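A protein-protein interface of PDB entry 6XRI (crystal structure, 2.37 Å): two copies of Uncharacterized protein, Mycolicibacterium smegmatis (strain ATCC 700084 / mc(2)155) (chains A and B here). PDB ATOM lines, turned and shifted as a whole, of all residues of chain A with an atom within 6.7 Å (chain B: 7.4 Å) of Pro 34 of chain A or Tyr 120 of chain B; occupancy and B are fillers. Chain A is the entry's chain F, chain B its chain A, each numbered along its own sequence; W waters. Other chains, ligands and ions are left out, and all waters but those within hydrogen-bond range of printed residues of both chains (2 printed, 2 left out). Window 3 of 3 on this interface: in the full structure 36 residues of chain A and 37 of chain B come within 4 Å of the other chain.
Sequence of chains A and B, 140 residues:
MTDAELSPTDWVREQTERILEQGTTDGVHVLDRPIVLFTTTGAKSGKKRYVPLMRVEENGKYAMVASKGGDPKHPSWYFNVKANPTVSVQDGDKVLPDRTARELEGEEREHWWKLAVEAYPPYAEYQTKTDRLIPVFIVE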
ATOM      1  N   ASP A  32      26.938   2.533  37.671  1.00  0.00           N
ATOM      2  CA  ASP A  32      27.716   1.303  37.563  1.00  0.00           C
ATOM      3  C   ASP A  32      28.463   1.312  36.234  1.00  0.00           C
ATOM      4  O   ASP A  32      28.009   1.924  35.267  1.00  0.00           O
ATOM      5  CB  ASP A  32      26.793   0.055  37.645  1.00  0.00           C
ATOM      6  CG  ASP A  32      26.161  -0.124  39.015  1.00  0.00           C
ATOM      7  OD1 ASP A  32      26.925  -0.273  39.991  1.00  0.00           O
ATOM      8  OD2 ASP A  32      24.910  -0.102  39.112  1.00  0.00           O
ATOM      9  N   ARG A  33      29.610   0.632  36.186  1.00  0.00           N
ATOM     10  CA  ARG A  33      30.237   0.319  34.903  1.00  0.00           C
ATOM     11  C   ARG A  33      29.195  -0.365  34.026  1.00  0.00           C
ATOM     12  O   ARG A  33      28.392  -1.146  34.550  1.00  0.00           O
ATOM     13  CB  ARG A  33      31.468  -0.562  35.119  1.00  0.00           C
ATOM     14  CG  ARG A  33      32.602   0.171  35.796  1.00  0.00           C
ATOM     15  CD  ARG A  33      33.845  -0.644  35.718  1.00  0.00           C
ATOM     16  NE  ARG A  33      34.869  -0.156  36.634  1.00  0.00           N
ATOM     17  CZ  ARG A  33      36.128  -0.590  36.668  1.00  0.00           C
ATOM     18  NH1 ARG A  33      36.540  -1.530  35.819  1.00  0.00           N
ATOM     19  NH2 ARG A  33      36.976  -0.083  37.565  1.00  0.00           N
ATOM     20  N   PRO A  34      29.182  -0.135  32.695  1.00  0.00           N
ATOM     21  CA  PRO A  34      30.257   0.543  31.935  1.00  0.00           C
ATOM     22  C   PRO A  34      30.065   2.033  31.716  1.00  0.00           C
ATOM     23  O   PRO A  34      30.667   2.613  30.817  1.00  0.00           O
ATOM     24  CB  PRO A  34      30.233  -0.168  30.582  1.00  0.00           C
ATOM     25  CG  PRO A  34      28.616  -0.515  30.385  1.00  0.00           C
ATOM     26  CD  PRO A  34      28.108  -0.705  31.841  1.00  0.00           C
ATOM     27  N   ILE A  35      29.214   2.644  32.515  1.00  0.00           N
ATOM     28  CA  ILE A  35      28.798   4.018  32.308  1.00  0.00           C
ATOM     29  C   ILE A  35      29.338   4.867  33.443  1.00  0.00           C
ATOM     30  O   ILE A  35      29.336   4.441  34.602  1.00  0.00           O
ATOM     31  CB  ILE A  35      27.265   4.111  32.236  1.00  0.00           C
ATOM     32  CG1 ILE A  35      26.739   3.346  31.024  1.00  0.00           C
ATOM     33  CG2 ILE A  35      26.852   5.520  32.150  1.00  0.00           C
ATOM     34  CD1 ILE A  35      25.235   3.211  30.966  1.00  0.00           C
ATOM     35  N   VAL A  36      29.783   6.076  33.103  1.00  0.00           N
ATOM     36  CA  VAL A  36      30.049   7.122  34.083  1.00  0.00           C
ATOM     37  C   VAL A  36      29.143   8.344  33.846  1.00  0.00           C
ATOM     38  O   VAL A  36      28.468   8.481  32.825  1.00  0.00           O
ATOM     39  CB  VAL A  36      31.527   7.531  34.067  1.00  0.00           C
ATOM     40  CG1 VAL A  36      32.383   6.332  34.497  1.00  0.00           C
ATOM     41  CG2 VAL A  36      31.876   8.025  32.668  1.00  0.00           C
ATOM     42  N   LEU A  53      27.803   8.987  29.949  1.00  0.00           N
ATOM     43  CA  LEU A  53      28.565   8.569  28.782  1.00  0.00           C
ATOM     44  C   LEU A  53      29.259   7.237  29.074  1.00  0.00           C
ATOM     45  O   LEU A  53      29.348   6.792  30.224  1.00  0.00           O
ATOM     46  CB  LEU A  53      29.594   9.642  28.386  1.00  0.00           C
ATOM     47  CG  LEU A  53      29.122  11.045  27.972  1.00  0.00           C
ATOM     48  CD1 LEU A  53      30.347  11.946  27.704  1.00  0.00           C
ATOM     49  CD2 LEU A  53      28.205  11.031  26.745  1.00  0.00           C
ATOM     50  N   MET A  54      29.757   6.598  28.014  1.00  0.00           N
ATOM     51  CA  MET A  54      30.553   5.386  28.183  1.00  0.00           C
ATOM     52  C   MET A  54      31.828   5.656  28.990  1.00  0.00           C
ATOM     53  O   MET A  54      32.551   6.635  28.780  1.00  0.00           O
ATOM     54  CB  MET A  54      30.920   4.775  26.818  1.00  0.00           C
ATOM     55  CG  MET A  54      29.738   4.382  25.933  1.00  0.00           C
ATOM     56  SD  MET A  54      28.701   3.114  26.652  1.00  0.00           S
ATOM     57  CE  MET A  54      29.949   1.861  26.958  1.00  0.00           C
ATOM     58  N   ARG A  55      32.115   4.755  29.904  1.00  0.00           N
ATOM     59  CA  ARG A  55      33.330   4.878  30.684  1.00  0.00           C
ATOM     60  C   ARG A  55      34.532   4.588  29.800  1.00  0.00           C
ATOM     61  O   ARG A  55      34.648   3.496  29.232  1.00  0.00           O
ATOM     62  CB  ARG A  55      33.269   3.918  31.865  1.00  0.00           C
ATOM     63  CG  ARG A  55      34.420   4.026  32.817  1.00  0.00           C
ATOM     64  CD  ARG A  55      34.383   2.992  33.927  1.00  0.00           C
ATOM     65  NE  ARG A  55      35.523   3.151  34.844  1.00  0.00           N
ATOM     66  CZ  ARG A  55      36.750   2.673  34.624  1.00  0.00           C
ATOM     67  NH1 ARG A  55      36.994   2.007  33.515  1.00  0.00           N
ATOM     68  NH2 ARG A  55      37.731   2.844  35.507  1.00  0.00           N
ATOM     69  N   VAL A  56      35.431   5.562  29.728  1.00  0.00           N
ATOM     70  CA  VAL A  56      36.703   5.458  29.036  1.00  0.00           C
ATOM     71  C   VAL A  56      37.723   6.080  29.977  1.00  0.00           C
ATOM     72  O   VAL A  56      37.760   7.305  30.128  1.00  0.00           O
ATOM     73  CB  VAL A  56      36.688   6.185  27.686  1.00  0.00           C
ATOM     74  CG1 VAL A  56      38.038   6.053  27.045  1.00  0.00           C
ATOM     75  CG2 VAL A  56      35.543   5.646  26.789  1.00  0.00           C
ATOM     76  N   ALA A 119      36.668   0.351  24.687  1.00  0.00           N
ATOM     77  CA  ALA A 119      35.552   0.275  25.627  1.00  0.00           C
ATOM     78  C   ALA A 119      34.199   0.129  24.928  1.00  0.00           C
ATOM     79  O   ALA A 119      33.312  -0.550  25.456  1.00  0.00           O
ATOM     80  CB  ALA A 119      35.531   1.512  26.535  1.00  0.00           C
ATOM     81  N   TYR A 120      33.992   0.762  23.778  1.00  0.00           N
ATOM     82  CA  TYR A 120      32.704   0.678  23.088  1.00  0.00           C
ATOM     83  C   TYR A 120      32.984   0.647  21.589  1.00  0.00           C
ATOM     84  O   TYR A 120      33.058   1.698  20.932  1.00  0.00           O
ATOM     85  CB  TYR A 120      31.774   1.833  23.483  1.00  0.00           C
ATOM     86  CG  TYR A 120      30.368   1.699  22.924  1.00  0.00           C
ATOM     87  CD1 TYR A 120      29.526   0.678  23.346  1.00  0.00           C
ATOM     88  CD2 TYR A 120      29.896   2.566  21.937  1.00  0.00           C
ATOM     89  CE1 TYR A 120      28.246   0.528  22.803  1.00  0.00           C
ATOM     90  CE2 TYR A 120      28.617   2.425  21.398  1.00  0.00           C
ATOM     91  CZ  TYR A 120      27.807   1.403  21.833  1.00  0.00           C
ATOM     92  OH  TYR A 120      26.554   1.256  21.306  1.00  0.00           O
ATOM     93  N   PRO A 121      33.139  -0.553  21.010  1.00  0.00           N
ATOM     94  CA  PRO A 121      33.602  -0.663  19.623  1.00  0.00           C
ATOM     95  C   PRO A 121      32.734   0.151  18.685  1.00  0.00           C
ATOM     96  O   PRO A 121      33.258   0.835  17.796  1.00  0.00           O
ATOM     97  CB  PRO A 121      33.493  -2.169  19.318  1.00  0.00           C
ATOM     98  CG  PRO A 121      33.622  -2.850  20.665  1.00  0.00           C
ATOM     99  CD  PRO A 121      32.894  -1.889  21.597  1.00  0.00           C
ATOM    100  N   PRO B  34      24.856   5.291  23.363  1.00  0.00           N
ATOM    101  CA  PRO B  34      24.153   4.025  23.659  1.00  0.00           C
ATOM    102  C   PRO B  34      23.507   3.914  25.028  1.00  0.00           C
ATOM    103  O   PRO B  34      23.328   2.797  25.510  1.00  0.00           O
ATOM    104  CB  PRO B  34      25.262   2.979  23.557  1.00  0.00           C
ATOM    105  CG  PRO B  34      26.514   3.743  24.088  1.00  0.00           C
ATOM    106  CD  PRO B  34      26.311   5.198  23.607  1.00  0.00           C
ATOM    107  N   ILE B  35      23.134   5.034  25.630  1.00  0.00           N
ATOM    108  CA  ILE B  35      22.694   5.050  27.017  1.00  0.00           C
ATOM    109  C   ILE B  35      21.296   5.644  27.112  1.00  0.00           C
ATOM    110  O   ILE B  35      20.904   6.524  26.336  1.00  0.00           O
ATOM    111  CB  ILE B  35      23.684   5.835  27.907  1.00  0.00           C
ATOM    112  CG1 ILE B  35      25.084   5.223  27.805  1.00  0.00           C
ATOM    113  CG2 ILE B  35      23.219   5.845  29.358  1.00  0.00           C
ATOM    114  CD1 ILE B  35      26.212   6.112  28.345  1.00  0.00           C
ATOM    115  N   PRO B  52      21.451   5.531  35.046  1.00  0.00           N
ATOM    116  CA  PRO B  52      21.812   5.381  33.631  1.00  0.00           C
ATOM    117  C   PRO B  52      22.262   3.956  33.324  1.00  0.00           C
ATOM    118  O   PRO B  52      23.118   3.388  34.005  1.00  0.00           O
ATOM    119  CB  PRO B  52      22.943   6.396  33.426  1.00  0.00           C
ATOM    120  CG  PRO B  52      23.409   6.888  34.849  1.00  0.00           C
ATOM    121  CD  PRO B  52      22.584   6.015  35.872  1.00  0.00           C
ATOM    122  N   LEU B  53      21.690   3.384  32.272  1.00  0.00           N
ATOM    123  CA  LEU B  53      21.985   2.018  31.876  1.00  0.00           C
ATOM    124  C   LEU B  53      22.144   1.936  30.363  1.00  0.00           C
ATOM    125  O   LEU B  53      21.697   2.812  29.623  1.00  0.00           O
ATOM    126  CB  LEU B  53      20.872   1.078  32.347  1.00  0.00           C
ATOM    127  CG  LEU B  53      20.643   0.914  33.851  1.00  0.00           C
ATOM    128  CD1 LEU B  53      19.495  -0.063  34.105  1.00  0.00           C
ATOM    129  CD2 LEU B  53      21.895   0.450  34.556  1.00  0.00           C
ATOM    130  N   MET B  54      22.783   0.861  29.908  1.00  0.00           N
ATOM    131  CA  MET B  54      22.873   0.611  28.478  1.00  0.00           C
ATOM    132  C   MET B  54      21.476   0.520  27.872  1.00  0.00           C
ATOM    133  O   MET B  54      20.551  -0.047  28.464  1.00  0.00           O
ATOM    134  CB  MET B  54      23.654  -0.676  28.212  1.00  0.00           C
ATOM    135  CG  MET B  54      25.102  -0.653  28.635  1.00  0.00           C
ATOM    136  SD  MET B  54      26.069   0.551  27.726  1.00  0.00           S
ATOM    137  CE  MET B  54      25.733   0.104  26.032  1.00  0.00           C
ATOM    138  N   ARG B  55      21.328   1.107  26.689  1.00  0.00           N
ATOM    139  CA  ARG B  55      20.066   1.112  25.965  1.00  0.00           C
ATOM    140  C   ARG B  55      19.832  -0.260  25.347  1.00  0.00           C
ATOM    141  O   ARG B  55      20.548  -0.666  24.429  1.00  0.00           O
ATOM    142  CB  ARG B  55      20.090   2.192  24.891  1.00  0.00           C
ATOM    143  CG  ARG B  55      18.801   2.275  24.101  1.00  0.00           C
ATOM    144  CD  ARG B  55      18.873   3.308  22.994  1.00  0.00           C
ATOM    145  NE  ARG B  55      17.601   3.407  22.280  1.00  0.00           N
ATOM    146  CZ  ARG B  55      17.233   2.595  21.295  1.00  0.00           C
ATOM    147  NH1 ARG B  55      18.047   1.619  20.907  1.00  0.00           N
ATOM    148  NH2 ARG B  55      16.055   2.756  20.699  1.00  0.00           N
ATOM    149  N   VAL B  56      18.834  -0.973  25.849  1.00  0.00           N
ATOM    150  CA  VAL B  56      18.389  -2.236  25.286  1.00  0.00           C
ATOM    151  C   VAL B  56      16.906  -2.036  25.052  1.00  0.00           C
ATOM    152  O   VAL B  56      16.152  -1.888  26.017  1.00  0.00           O
ATOM    153  CB  VAL B  56      18.652  -3.417  26.226  1.00  0.00           C
ATOM    154  CG1 VAL B  56      18.182  -4.690  25.595  1.00  0.00           C
ATOM    155  CG2 VAL B  56      20.145  -3.524  26.561  1.00  0.00           C
ATOM    156  N   SER B  67      23.317  -5.691  36.465  1.00  0.00           N
ATOM    157  CA  SER B  67      24.693  -6.065  36.754  1.00  0.00           C
ATOM    158  C   SER B  67      25.414  -4.914  37.445  1.00  0.00           C
ATOM    159  O   SER B  67      24.899  -3.801  37.558  1.00  0.00           O
ATOM    160  CB  SER B  67      25.453  -6.447  35.490  1.00  0.00           C
ATOM    161  OG  SER B  67      26.841  -6.564  35.785  1.00  0.00           O
ATOM    162  N   LYS B  68      26.637  -5.180  37.892  1.00  0.00           N
ATOM    163  CA  LYS B  68      27.417  -4.168  38.601  1.00  0.00           C
ATOM    164  C   LYS B  68      28.846  -4.157  38.078  1.00  0.00           C
ATOM    165  O   LYS B  68      29.819  -4.083  38.831  1.00  0.00           O
ATOM    166  CB  LYS B  68      27.391  -4.397  40.110  1.00  0.00           C
ATOM    167  CG  LYS B  68      27.653  -3.145  40.907  1.00  0.00           C
ATOM    168  CD  LYS B  68      27.832  -3.411  42.376  1.00  0.00           C
ATOM    169  CE  LYS B  68      28.409  -2.157  43.020  1.00  0.00           C
ATOM    170  NZ  LYS B  68      27.554  -0.932  42.775  1.00  0.00           N
ATOM    171  N   GLY B  69      28.979  -4.222  36.759  1.00  0.00           N
ATOM    172  CA  GLY B  69      30.288  -4.101  36.170  1.00  0.00           C
ATOM    173  C   GLY B  69      31.174  -5.288  36.422  1.00  0.00           C
ATOM    174  O   GLY B  69      32.397  -5.151  36.392  1.00  0.00           O
ATOM    175  N   TRP B 113      17.921 -11.160  27.342  1.00  0.00           N
ATOM    176  CA  TRP B 113      19.355 -11.310  27.554  1.00  0.00           C
ATOM    177  C   TRP B 113      20.114 -11.414  26.237  1.00  0.00           C
ATOM    178  O   TRP B 113      21.259 -10.956  26.133  1.00  0.00           O
ATOM    179  CB  TRP B 113      19.638 -12.534  28.396  1.00  0.00           C
ATOM    180  CG  TRP B 113      21.093 -12.753  28.618  1.00  0.00           C
ATOM    181  CD1 TRP B 113      21.876 -13.703  28.036  1.00  0.00           C
ATOM    182  CD2 TRP B 113      21.952 -12.006  29.487  1.00  0.00           C
ATOM    183  NE1 TRP B 113      23.161 -13.618  28.513  1.00  0.00           N
ATOM    184  CE2 TRP B 113      23.237 -12.569  29.390  1.00  0.00           C
ATOM    185  CE3 TRP B 113      21.758 -10.913  30.334  1.00  0.00           C
ATOM    186  CZ2 TRP B 113      24.322 -12.082  30.111  1.00  0.00           C
ATOM    187  CZ3 TRP B 113      22.836 -10.437  31.054  1.00  0.00           C
ATOM    188  CH2 TRP B 113      24.099 -11.021  30.940  1.00  0.00           C
ATOM    189  N   LYS B 114      19.509 -12.043  25.233  1.00  0.00           N
ATOM    190  CA  LYS B 114      20.094 -12.032  23.899  1.00  0.00           C
ATOM    191  C   LYS B 114      20.221 -10.605  23.384  1.00  0.00           C
ATOM    192  O   LYS B 114      21.289 -10.186  22.920  1.00  0.00           O
ATOM    193  CB  LYS B 114      19.237 -12.891  22.971  1.00  0.00           C
ATOM    194  CG  LYS B 114      19.460 -12.649  21.505  1.00  0.00           C
ATOM    195  CD  LYS B 114      20.836 -13.124  21.065  1.00  0.00           C
ATOM    196  CE  LYS B 114      20.959 -13.165  19.526  1.00  0.00           C
ATOM    197  NZ  LYS B 114      21.683 -11.973  18.983  1.00  0.00           N
ATOM    198  N   LEU B 115      19.138  -9.831  23.479  1.00  0.00           N
ATOM    199  CA  LEU B 115      19.185  -8.461  22.981  1.00  0.00           C
ATOM    200  C   LEU B 115      20.228  -7.645  23.726  1.00  0.00           C
ATOM    201  O   LEU B 115      20.910  -6.807  23.127  1.00  0.00           O
ATOM    202  CB  LEU B 115      17.823  -7.797  23.118  1.00  0.00           C
ATOM    203  CG  LEU B 115      16.650  -8.442  22.385  1.00  0.00           C
ATOM    204  CD1 LEU B 115      15.596  -7.358  22.069  1.00  0.00           C
ATOM    205  CD2 LEU B 115      17.064  -9.136  21.128  1.00  0.00           C
ATOM    206  N   ALA B 116      20.350  -7.869  25.040  1.00  0.00           N
ATOM    207  CA  ALA B 116      21.328  -7.153  25.856  1.00  0.00           C
ATOM    208  C   ALA B 116      22.755  -7.500  25.444  1.00  0.00           C
ATOM    209  O   ALA B 116      23.606  -6.611  25.312  1.00  0.00           O
ATOM    210  CB  ALA B 116      21.108  -7.472  27.335  1.00  0.00           C
ATOM    211  N   VAL B 117      23.034  -8.785  25.228  1.00  0.00           N
ATOM    212  CA  VAL B 117      24.363  -9.177  24.776  1.00  0.00           C
ATOM    213  C   VAL B 117      24.621  -8.628  23.385  1.00  0.00           C
ATOM    214  O   VAL B 117      25.761  -8.273  23.042  1.00  0.00           O
ATOM    215  CB  VAL B 117      24.500 -10.710  24.821  1.00  0.00           C
ATOM    216  CG1 VAL B 117      25.780 -11.142  24.090  1.00  0.00           C
ATOM    217  CG2 VAL B 117      24.475 -11.202  26.274  1.00  0.00           C
ATOM    218  N   GLU B 118      23.568  -8.546  22.565  1.00  0.00           N
ATOM    219  CA  GLU B 118      23.651  -7.893  21.265  1.00  0.00           C
ATOM    220  C   GLU B 118      24.089  -6.446  21.419  1.00  0.00           C
ATOM    221  O   GLU B 118      25.123  -6.052  20.877  1.00  0.00           O
ATOM    222  CB  GLU B 118      22.308  -7.970  20.547  1.00  0.00           C
ATOM    223  CG  GLU B 118      22.284  -7.220  19.205  1.00  0.00           C
ATOM    224  CD  GLU B 118      22.775  -8.063  18.043  1.00  0.00           C
ATOM    225  OE1 GLU B 118      23.274  -9.179  18.289  1.00  0.00           O
ATOM    226  OE2 GLU B 118      22.662  -7.604  16.885  1.00  0.00           O
ATOM    227  N   ALA B 119      23.450  -5.705  22.320  1.00  0.00           N
ATOM    228  CA  ALA B 119      23.797  -4.294  22.471  1.00  0.00           C
ATOM    229  C   ALA B 119      25.140  -4.096  23.176  1.00  0.00           C
ATOM    230  O   ALA B 119      25.923  -3.218  22.790  1.00  0.00           O
ATOM    231  CB  ALA B 119      22.690  -3.572  23.229  1.00  0.00           C
ATOM    232  N   TYR B 120      25.415  -4.867  24.226  1.00  0.00           N
ATOM    233  CA  TYR B 120      26.642  -4.697  25.005  1.00  0.00           C
ATOM    234  C   TYR B 120      27.223  -6.082  25.264  1.00  0.00           C
ATOM    235  O   TYR B 120      26.886  -6.734  26.263  1.00  0.00           O
ATOM    236  CB  TYR B 120      26.382  -3.927  26.309  1.00  0.00           C
ATOM    237  CG  TYR B 120      27.657  -3.601  27.059  1.00  0.00           C
ATOM    238  CD1 TYR B 120      28.648  -2.816  26.484  1.00  0.00           C
ATOM    239  CD2 TYR B 120      27.876  -4.097  28.333  1.00  0.00           C
ATOM    240  CE1 TYR B 120      29.822  -2.541  27.157  1.00  0.00           C
ATOM    241  CE2 TYR B 120      29.046  -3.841  29.014  1.00  0.00           C
ATOM    242  CZ  TYR B 120      30.026  -3.064  28.436  1.00  0.00           C
ATOM    243  OH  TYR B 120      31.196  -2.841  29.155  1.00  0.00           O
ATOM    244  N   PRO B 121      28.103  -6.567  24.385  1.00  0.00           N
ATOM    245  CA  PRO B 121      28.538  -7.969  24.487  1.00  0.00           C
ATOM    246  C   PRO B 121      29.162  -8.268  25.838  1.00  0.00           C
ATOM    247  O   PRO B 121      29.003  -9.383  26.358  1.00  0.00           O
ATOM    248  CB  PRO B 121      29.566  -8.118  23.353  1.00  0.00           C
ATOM    249  CG  PRO B 121      29.122  -7.117  22.321  1.00  0.00           C
ATOM    250  CD  PRO B 121      28.722  -5.907  23.216  1.00  0.00           C
ATOM    251  N   PRO B 122      29.904  -7.327  26.432  1.00  0.00           N
ATOM    252  CA  PRO B 122      30.573  -7.639  27.714  1.00  0.00           C
ATOM    253  C   PRO B 122      29.597  -8.023  28.830  1.00  0.00           C
ATOM    254  O   PRO B 122      30.015  -8.615  29.837  1.00  0.00           O
ATOM    255  CB  PRO B 122      31.356  -6.353  28.039  1.00  0.00           C
ATOM    256  CG  PRO B 122      31.590  -5.693  26.701  1.00  0.00           C
ATOM    257  CD  PRO B 122      30.314  -6.013  25.899  1.00  0.00           C
ATOM    258  N   TYR B 123      28.305  -7.745  28.678  1.00  0.00           N
ATOM    259  CA  TYR B 123      27.331  -8.331  29.593  1.00  0.00           C
ATOM    260  C   TYR B 123      27.566  -9.830  29.784  1.00  0.00           C
ATOM    261  O   TYR B 123      27.445 -10.344  30.901  1.00  0.00           O
ATOM    262  CB  TYR B 123      25.911  -8.092  29.083  1.00  0.00           C
ATOM    263  CG  TYR B 123      25.311  -6.765  29.455  1.00  0.00           C
ATOM    264  CD1 TYR B 123      25.496  -6.214  30.713  1.00  0.00           C
ATOM    265  CD2 TYR B 123      24.541  -6.068  28.541  1.00  0.00           C
ATOM    266  CE1 TYR B 123      24.936  -4.997  31.037  1.00  0.00           C
ATOM    267  CE2 TYR B 123      23.972  -4.860  28.857  1.00  0.00           C
ATOM    268  CZ  TYR B 123      24.164  -4.327  30.098  1.00  0.00           C
ATOM    269  OH  TYR B 123      23.588  -3.105  30.344  1.00  0.00           O
ATOM    270  N   ALA B 124      27.878 -10.552  28.698  1.00  0.00           N
ATOM    271  CA  ALA B 124      28.163 -11.981  28.806  1.00  0.00           C
ATOM    272  C   ALA B 124      29.425 -12.230  29.622  1.00  0.00           C
ATOM    273  O   ALA B 124      29.492 -13.187  30.399  1.00  0.00           O
ATOM    274  CB  ALA B 124      28.297 -12.604  27.416  1.00  0.00           C
ATOM    275  N   GLU B 125      30.436 -11.375  29.474  1.00  0.00           N
ATOM    276  CA  GLU B 125      31.623 -11.514  30.309  1.00  0.00           C
ATOM    277  C   GLU B 125      31.283 -11.348  31.787  1.00  0.00           C
ATOM    278  O   GLU B 125      31.876 -12.010  32.648  1.00  0.00           O
ATOM    279  CB  GLU B 125      32.680 -10.492  29.896  1.00  0.00           C
ATOM    280  CG  GLU B 125      33.090 -10.559  28.446  1.00  0.00           C
ATOM    281  CD  GLU B 125      33.756 -11.880  28.075  1.00  0.00           C
ATOM    282  OE1 GLU B 125      33.787 -12.205  26.868  1.00  0.00           O
ATOM    283  OE2 GLU B 125      34.245 -12.593  28.980  1.00  0.00           O
ATOM    284  N   TYR B 126      30.359 -10.431  32.099  1.00  0.00           N
ATOM    285  CA  TYR B 126      29.883 -10.261  33.469  1.00  0.00           C
ATOM    286  C   TYR B 126      29.295 -11.560  34.013  1.00  0.00           C
ATOM    287  O   TYR B 126      29.625 -11.983  35.129  1.00  0.00           O
ATOM    288  CB  TYR B 126      28.828  -9.148  33.536  1.00  0.00           C
ATOM    289  CG  TYR B 126      29.303  -7.748  33.186  1.00  0.00           C
ATOM    290  CD1 TYR B 126      30.648  -7.479  32.977  1.00  0.00           C
ATOM    291  CD2 TYR B 126      28.388  -6.693  33.070  1.00  0.00           C
ATOM    292  CE1 TYR B 126      31.070  -6.212  32.657  1.00  0.00           C
ATOM    293  CE2 TYR B 126      28.800  -5.420  32.751  1.00  0.00           C
ATOM    294  CZ  TYR B 126      30.144  -5.185  32.545  1.00  0.00           C
ATOM    295  OH  TYR B 126      30.572  -3.919  32.222  1.00  0.00           O
HETATM  296  O   HOH W   1      26.465  -3.026  34.925  1.00  0.00           O
HETATM  297  O   HOH W   2      32.593  -1.138  27.900  1.00  0.00           O
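NZ of Lys 68 of chain B lies within salt-bridge range of OD1 of Asp 32 of chain A (2.9 Å).
O of Pro 34 of chain B is in hydrogen-bond range of N of Arg 55 of chain B.
O of Pro 34 of chain A is in hydrogen-bond range of N of Arg 55 of chain A (2.7 Å).
N of Leu 53 of chain A sits at hydrogen-bond distance from O of Val 36 of chain A (3.0 Å).
N of Gly 69 of chain B lies within hydrogen-bond range of OG of Ser 67 of chain B (3.3 Å).
The side-chain hydroxyl of Tyr 120 of chain B sits at hydrogen-bond distance from the side-chain hydroxyl of Tyr 126 of chain B (3.3 Å).
Among the printed residues, pairs that only touch across the chains: Arg 33 of chain A with Gly 69 of chain B (3.8 Å), Pro 34 of chain A with Met 54 of chain B (3.8 Å), Pro 34 of chain A with Tyr 120 of chain B (3.2 Å), Ile 35 of chain A with Ile 35 of chain B (3.7 Å), Ile 35 of chain A with Pro 52 of chain B (3.7 Å), Ile 35 of chain A with Leu 53 of chain B (3.4 Å), Ile 35 of chain A with Met 54 of chain B (3.6 Å), Leu 53 of chain A with Ile 35 of chain B (3.3 Å), Met 54 of chain A with Pro 34 of chain B (3.4 Å), Met 54 of chain A with Ile 35 of chain B (3.6 Å), Met 54 of chain A with Met 54 of chain B (3.8 Å) and Tyr 120 of chain A with Pro 34 of chain B (3.1 Å).
Of the printed residues of chain B, Arg 33 of chain A touches Gly 69 (3.8 Å).
Pro 34 of chain A touches just these residues of chain B: Met 54 and Tyr 120.
Ala 119 of chain A touches none of the printed residues of chain B.
Printed residues of chain A within 4 Å of Lys 68 of chain B: Asp 32.
Val 117 of chain B touches none of the printed residues of chain A.
Tyr 120 of chain B touches one residue of chain A.
The nearest residue of chain B that does not touch Pro 34 of chain A is Tyr 126 of chain B (4.1 Å).
Of the 12 printed residues of chain A, 7 touch a printed residue of chain B.
Printed residues of chain B that touch a printed residue of chain A: Pro 34, Ile 35, Pro 52, Leu 53, Met 54, Lys 68, Gly 69 and Tyr 120.
Hydrophobic or aromatic side chains of chain B within 4 Å of the printed part of chain A: Pro 34, Ile 35, Met 54 and Tyr 120.
Along chain B the printed residues that touch a printed residue of chain A span positions 34 to 120.
Among the printed residues, 13 pairs touch across the chains.
Among the printed residues, Asp or Glu carboxylates within 4 Å of a Lys or Arg side-chain nitrogen of the other chain: Asp 32 of chain A with Lys 68 of chain B.
Pro 34 of chain A touches Met 54 of chain B, and with the chains exchanged Met 54 of chain A touches Pro 34 of chain B.
Ile 35 of chain A touches its own counterpart, Ile 35 of chain B.
Ile 35 of chain A touches Met 54 of chain B, and with the chains exchanged Met 54 of chain A touches Ile 35 of chain B.
Met 54 of chain A touches its own counterpart, Met 54 of chain B.
Of the 13 pairs that touch across the chains among the printed residues, 10 have their exchanged pair printed and touching as well.
Water W2 bridges the side-chain hydroxyl of Tyr 120 of chain B and the backbone carbonyl oxygen of Ala 119 of chain A.
Water W1 lies within hydrogen-bond range of the backbone carbonyl oxygen (O) of Arg 33 of chain A (2.7 Å), the backbone carbonyl oxygen (O) of Ser 67 of chain B (3.2 Å) and the backbone NH (N) of Gly 69 of chain B (3.3 Å).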
